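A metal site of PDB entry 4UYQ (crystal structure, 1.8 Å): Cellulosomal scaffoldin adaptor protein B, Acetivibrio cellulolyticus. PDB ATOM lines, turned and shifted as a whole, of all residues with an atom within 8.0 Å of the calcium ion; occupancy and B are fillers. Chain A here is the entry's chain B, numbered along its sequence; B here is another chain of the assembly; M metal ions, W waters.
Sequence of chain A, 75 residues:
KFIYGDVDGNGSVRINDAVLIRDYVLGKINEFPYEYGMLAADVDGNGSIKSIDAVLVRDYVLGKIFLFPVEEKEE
The side-chain carboxylate (OD1) of Asp 6 lies close to the backbone NH (N) of Gly 9 (3.2 Å). The side-chain carboxylate of Asp 6 sits at hydrogen-bond distance from the backbone NH of Gly 11 (2.8 Å). The side-chain amide nitrogen (ND2) of Asn 10 sits close to the guanidinium group (NH1) of Arg 14 (3.4 Å). The side-chain amide nitrogen (ND2) of Asn 16 is in hydrogen-bond range of the side-chain carboxylate (OD2) of Asp 8. The backbone NH (N) of Arg 14 lies close to the side-chain carboxylate (OD2) of Asp 17, at 2.8 Å. The backbone NH (N) of Val 7 lies close to the side-chain carboxylate (OD1) of Asp 17.
The calcium ion is bound by O of Ser 12 (2.3 Å), water W1 (2.4 Å), OD1 of Asp 6 (2.4 Å), OD1 of Asn 10 (2.4 Å), OD1 of Asp 8 (2.4 Å), OD2 of Asp 17 (2.4 Å) and OD1 of Asp 17 (2.6 Å).
Of the 20 residues printed, 5 come within 4 Å of the calcium ion.
Water W1 lies within hydrogen-bond range of OD1 of Asn 16, OD2 of Asp 8 and ND2 of Asn 10.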
ATOM      1  N   ILE A   3      -6.231 -23.544  -5.207  1.00  0.00           N
ATOM      2  CA  ILE A   3      -6.422 -24.683  -6.104  1.00  0.00           C
ATOM      3  C   ILE A   3      -5.927 -24.289  -7.496  1.00  0.00           C
ATOM      4  O   ILE A   3      -6.283 -23.178  -7.974  1.00  0.00           O
ATOM      5  CB  ILE A   3      -7.952 -24.986  -6.179  1.00  0.00           C
ATOM      6  CG1 ILE A   3      -8.430 -25.455  -4.775  1.00  0.00           C
ATOM      7  CG2 ILE A   3      -8.313 -26.001  -7.214  1.00  0.00           C
ATOM      8  CD1 ILE A   3      -9.917 -25.206  -4.614  1.00  0.00           C
ATOM      9  N   GLY A   5      -5.759 -23.913 -11.302  1.00  0.00           N
ATOM     10  CA  GLY A   5      -6.925 -23.714 -12.198  1.00  0.00           C
ATOM     11  C   GLY A   5      -7.993 -22.728 -11.754  1.00  0.00           C
ATOM     12  O   GLY A   5      -8.804 -22.299 -12.527  1.00  0.00           O
ATOM     13  N   ASP A   6      -8.033 -22.402 -10.464  1.00  0.00           N
ATOM     14  CA  ASP A   6      -9.071 -21.580  -9.898  1.00  0.00           C
ATOM     15  C   ASP A   6      -8.588 -20.137  -9.812  1.00  0.00           C
ATOM     16  O   ASP A   6      -8.212 -19.681  -8.739  1.00  0.00           O
ATOM     17  CB  ASP A   6      -9.491 -22.038  -8.510  1.00  0.00           C
ATOM     18  CG  ASP A   6     -10.552 -21.141  -7.861  1.00  0.00           C
ATOM     19  OD1 ASP A   6     -11.331 -20.515  -8.567  1.00  0.00           O
ATOM     20  OD2 ASP A   6     -10.624 -21.053  -6.583  1.00  0.00           O
ATOM     21  N   VAL A   7      -8.607 -19.456 -10.922  1.00  0.00           N
ATOM     22  CA  VAL A   7      -8.039 -18.083 -11.059  1.00  0.00           C
ATOM     23  C   VAL A   7      -8.994 -16.998 -10.549  1.00  0.00           C
ATOM     24  O   VAL A   7      -8.576 -15.884 -10.325  1.00  0.00           O
ATOM     25  CB  VAL A   7      -7.539 -17.795 -12.488  1.00  0.00           C
ATOM     26  CG1 VAL A   7      -6.570 -18.873 -12.949  1.00  0.00           C
ATOM     27  CG2 VAL A   7      -8.685 -17.708 -13.459  1.00  0.00           C
ATOM     28  N   ASP A   8     -10.264 -17.299 -10.352  1.00  0.00           N
ATOM     29  CA  ASP A   8     -11.184 -16.314  -9.738  1.00  0.00           C
ATOM     30  C   ASP A   8     -11.390 -16.475  -8.260  1.00  0.00           C
ATOM     31  O   ASP A   8     -12.126 -15.700  -7.631  1.00  0.00           O
ATOM     32  CB  ASP A   8     -12.505 -16.197 -10.495  1.00  0.00           C
ATOM     33  CG  ASP A   8     -13.454 -17.349 -10.249  1.00  0.00           C
ATOM     34  OD1 ASP A   8     -13.106 -18.400  -9.640  1.00  0.00           O
ATOM     35  OD2 ASP A   8     -14.619 -17.177 -10.679  1.00  0.00           O
ATOM     36  N   GLY A   9     -10.797 -17.519  -7.705  1.00  0.00           N
ATOM     37  CA  GLY A   9     -10.781 -17.799  -6.247  1.00  0.00           C
ATOM     38  C   GLY A   9     -12.104 -18.185  -5.636  1.00  0.00           C
ATOM     39  O   GLY A   9     -12.354 -18.031  -4.420  1.00  0.00           O
ATOM     40  N   ASN A  10     -13.025 -18.671  -6.433  1.00  0.00           N
ATOM     41  CA  ASN A  10     -14.232 -19.133  -5.858  1.00  0.00           C
ATOM     42  C   ASN A  10     -14.176 -20.511  -5.258  1.00  0.00           C
ATOM     43  O   ASN A  10     -15.210 -21.019  -4.841  1.00  0.00           O
ATOM     44  CB  ASN A  10     -15.425 -19.030  -6.871  1.00  0.00           C
ATOM     45  CG  ASN A  10     -15.482 -20.155  -7.854  1.00  0.00           C
ATOM     46  OD1 ASN A  10     -14.467 -20.731  -8.253  1.00  0.00           O
ATOM     47  ND2 ASN A  10     -16.670 -20.438  -8.334  1.00  0.00           N
ATOM     48  N   GLY A  11     -13.081 -21.206  -5.344  1.00  0.00           N
ATOM     49  CA  GLY A  11     -12.994 -22.586  -4.817  1.00  0.00           C
ATOM     50  C   GLY A  11     -13.250 -23.781  -5.719  1.00  0.00           C
ATOM     51  O   GLY A  11     -13.199 -24.920  -5.240  1.00  0.00           O
ATOM     52  N   SER A  12     -13.526 -23.528  -7.008  1.00  0.00           N
ATOM     53  CA  SER A  12     -13.876 -24.544  -7.999  1.00  0.00           C
ATOM     54  C   SER A  12     -13.175 -24.170  -9.267  1.00  0.00           C
ATOM     55  O   SER A  12     -13.109 -22.963  -9.596  1.00  0.00           O
ATOM     56  CB  SER A  12     -15.396 -24.495  -8.335  1.00  0.00           C
ATOM     57  OG  SER A  12     -16.094 -24.906  -7.220  1.00  0.00           O
ATOM     58  N   VAL A  13     -12.698 -25.188  -9.994  1.00  0.00           N
ATOM     59  CA  VAL A  13     -12.179 -25.014 -11.330  1.00  0.00           C
ATOM     60  C   VAL A  13     -13.383 -25.167 -12.299  1.00  0.00           C
ATOM     61  O   VAL A  13     -14.087 -26.182 -12.306  1.00  0.00           O
ATOM     62  CB  VAL A  13     -11.118 -26.032 -11.710  1.00  0.00           C
ATOM     63  CG1 VAL A  13     -10.643 -25.797 -13.114  1.00  0.00           C
ATOM     64  CG2 VAL A  13      -9.946 -25.927 -10.749  1.00  0.00           C
ATOM     65  N   ARG A  14     -13.679 -24.093 -13.017  1.00  0.00           N
ATOM     66  CA  ARG A  14     -14.802 -24.027 -13.950  1.00  0.00           C
ATOM     67  C   ARG A  14     -14.399 -23.421 -15.269  1.00  0.00           C
ATOM     68  O   ARG A  14     -13.277 -22.874 -15.470  1.00  0.00           O
ATOM     69  CB  ARG A  14     -15.954 -23.151 -13.349  1.00  0.00           C
ATOM     70  CG  ARG A  14     -16.490 -23.547 -12.012  1.00  0.00           C
ATOM     71  CD  ARG A  14     -17.599 -22.599 -11.591  1.00  0.00           C
ATOM     72  NE  ARG A  14     -18.248 -22.985 -10.335  1.00  0.00           N
ATOM     73  CZ  ARG A  14     -19.207 -22.300  -9.739  1.00  0.00           C
ATOM     74  NH1 ARG A  14     -19.504 -21.105 -10.153  1.00  0.00           N
ATOM     75  NH2 ARG A  14     -19.753 -22.771  -8.634  1.00  0.00           N
ATOM     76  N   ILE A  15     -15.337 -23.479 -16.228  1.00  0.00           N
ATOM     77  CA  ILE A  15     -15.073 -22.964 -17.554  1.00  0.00           C
ATOM     78  C   ILE A  15     -14.684 -21.510 -17.535  1.00  0.00           C
ATOM     79  O   ILE A  15     -13.899 -21.096 -18.336  1.00  0.00           O
ATOM     80  CB  ILE A  15     -16.320 -23.234 -18.524  1.00  0.00           C
ATOM     81  CG1 ILE A  15     -15.905 -23.021 -19.983  1.00  0.00           C
ATOM     82  CG2 ILE A  15     -17.499 -22.368 -18.147  1.00  0.00           C
ATOM     83  CD1 ILE A  15     -14.732 -23.881 -20.392  1.00  0.00           C
ATOM     84  N   ASN A  16     -15.240 -20.695 -16.602  1.00  0.00           N
ATOM     85  CA  ASN A  16     -14.897 -19.247 -16.650  1.00  0.00           C
ATOM     86  C   ASN A  16     -13.439 -19.004 -16.252  1.00  0.00           C
ATOM     87  O   ASN A  16     -12.826 -18.042 -16.663  1.00  0.00           O
ATOM     88  CB  ASN A  16     -15.815 -18.405 -15.768  1.00  0.00           C
ATOM     89  CG  ASN A  16     -15.551 -18.611 -14.275  1.00  0.00           C
ATOM     90  OD1 ASN A  16     -15.636 -19.724 -13.790  1.00  0.00           O
ATOM     91  ND2 ASN A  16     -15.313 -17.553 -13.569  1.00  0.00           N
ATOM     92  N   ASP A  17     -12.860 -19.939 -15.484  1.00  0.00           N
ATOM     93  CA  ASP A  17     -11.450 -19.848 -15.106  1.00  0.00           C
ATOM     94  C   ASP A  17     -10.616 -20.004 -16.404  1.00  0.00           C
ATOM     95  O   ASP A  17      -9.661 -19.272 -16.595  1.00  0.00           O
ATOM     96  CB  ASP A  17     -11.068 -20.947 -14.063  1.00  0.00           C
ATOM     97  CG  ASP A  17     -11.778 -20.744 -12.734  1.00  0.00           C
ATOM     98  OD1 ASP A  17     -11.592 -19.695 -12.042  1.00  0.00           O
ATOM     99  OD2 ASP A  17     -12.465 -21.663 -12.280  1.00  0.00           O
ATOM    100  N   ALA A  18     -11.008 -20.925 -17.303  1.00  0.00           N
ATOM    101  CA  ALA A  18     -10.291 -21.113 -18.549  1.00  0.00           C
ATOM    102  C   ALA A  18     -10.365 -19.843 -19.382  1.00  0.00           C
ATOM    103  O   ALA A  18      -9.359 -19.360 -19.901  1.00  0.00           O
ATOM    104  CB  ALA A  18     -10.831 -22.322 -19.326  1.00  0.00           C
ATOM    105  N   LEU A  20     -11.069 -16.697 -18.385  1.00  0.00           N
ATOM    106  CA  LEU A  20     -10.235 -15.662 -17.743  1.00  0.00           C
ATOM    107  C   LEU A  20      -8.745 -15.761 -18.119  1.00  0.00           C
ATOM    108  O   LEU A  20      -8.134 -14.735 -18.453  1.00  0.00           O
ATOM    109  CB  LEU A  20     -10.415 -15.628 -16.233  1.00  0.00           C
ATOM    110  CG  LEU A  20     -11.765 -15.076 -15.697  1.00  0.00           C
ATOM    111  CD1 LEU A  20     -11.887 -15.398 -14.231  1.00  0.00           C
ATOM    112  CD2 LEU A  20     -11.918 -13.553 -15.972  1.00  0.00           C
ATOM    113  N   TYR A  34      -8.432 -12.201  -7.950  1.00  0.00           N
ATOM    114  CA  TYR A  34      -8.035 -13.137  -6.902  1.00  0.00           C
ATOM    115  C   TYR A  34      -6.559 -13.033  -6.569  1.00  0.00           C
ATOM    116  O   TYR A  34      -5.686 -13.046  -7.459  1.00  0.00           O
ATOM    117  CB  TYR A  34      -8.309 -14.530  -7.373  1.00  0.00           C
ATOM    118  CG  TYR A  34      -7.984 -15.675  -6.426  1.00  0.00           C
ATOM    119  CD1 TYR A  34      -8.310 -15.622  -5.078  1.00  0.00           C
ATOM    120  CD2 TYR A  34      -7.449 -16.864  -6.935  1.00  0.00           C
ATOM    121  CE1 TYR A  34      -8.088 -16.700  -4.265  1.00  0.00           C
ATOM    122  CE2 TYR A  34      -7.258 -17.971  -6.145  1.00  0.00           C
ATOM    123  CZ  TYR A  34      -7.521 -17.870  -4.795  1.00  0.00           C
ATOM    124  OH  TYR A  34      -7.368 -18.989  -3.950  1.00  0.00           O
ATOM    125  N   VAL A  57      -6.844 -25.927 -18.429  1.00  0.00           N
ATOM    126  CA  VAL A  57      -8.030 -25.695 -17.537  1.00  0.00           C
ATOM    127  C   VAL A  57      -9.353 -26.199 -18.216  1.00  0.00           C
ATOM    128  O   VAL A  57     -10.147 -26.926 -17.574  1.00  0.00           O
ATOM    129  CB  VAL A  57      -8.145 -24.265 -17.016  1.00  0.00           C
ATOM    130  CG1 VAL A  57      -9.446 -24.100 -16.183  1.00  0.00           C
ATOM    131  CG2 VAL A  57      -6.928 -23.881 -16.223  1.00  0.00           C
ATOM    132  N   TYR B 122     -22.044 -18.860 -17.782  1.00  0.00           N
ATOM    133  CA  TYR B 122     -21.475 -17.537 -17.544  1.00  0.00           C
ATOM    134  C   TYR B 122     -21.913 -16.461 -18.592  1.00  0.00           C
ATOM    135  O   TYR B 122     -21.929 -16.680 -19.787  1.00  0.00           O
ATOM    136  CB  TYR B 122     -19.961 -17.586 -17.413  1.00  0.00           C
ATOM    137  CG  TYR B 122     -19.552 -18.048 -16.076  1.00  0.00           C
ATOM    138  CD1 TYR B 122     -19.532 -19.438 -15.761  1.00  0.00           C
ATOM    139  CD2 TYR B 122     -19.192 -17.152 -15.095  1.00  0.00           C
ATOM    140  CE1 TYR B 122     -19.149 -19.868 -14.507  1.00  0.00           C
ATOM    141  CE2 TYR B 122     -18.806 -17.573 -13.812  1.00  0.00           C
ATOM    142  CZ  TYR B 122     -18.809 -18.952 -13.515  1.00  0.00           C
ATOM    143  OH  TYR B 122     -18.482 -19.415 -12.247  1.00  0.00           O
ATOM    144  N   GLY B 125     -16.613 -13.379 -18.120  1.00  0.00           N
ATOM    145  CA  GLY B 125     -15.556 -14.112 -17.410  1.00  0.00           C
ATOM    146  C   GLY B 125     -15.730 -14.193 -15.918  1.00  0.00           C
ATOM    147  O   GLY B 125     -15.300 -15.145 -15.304  1.00  0.00           O
HETATM  148 CA    CA M   1     -13.065 -20.730 -10.160  1.00  0.00          CA
HETATM  149  O   HOH W   1     -15.112 -20.273 -11.232  1.00  0.00           O
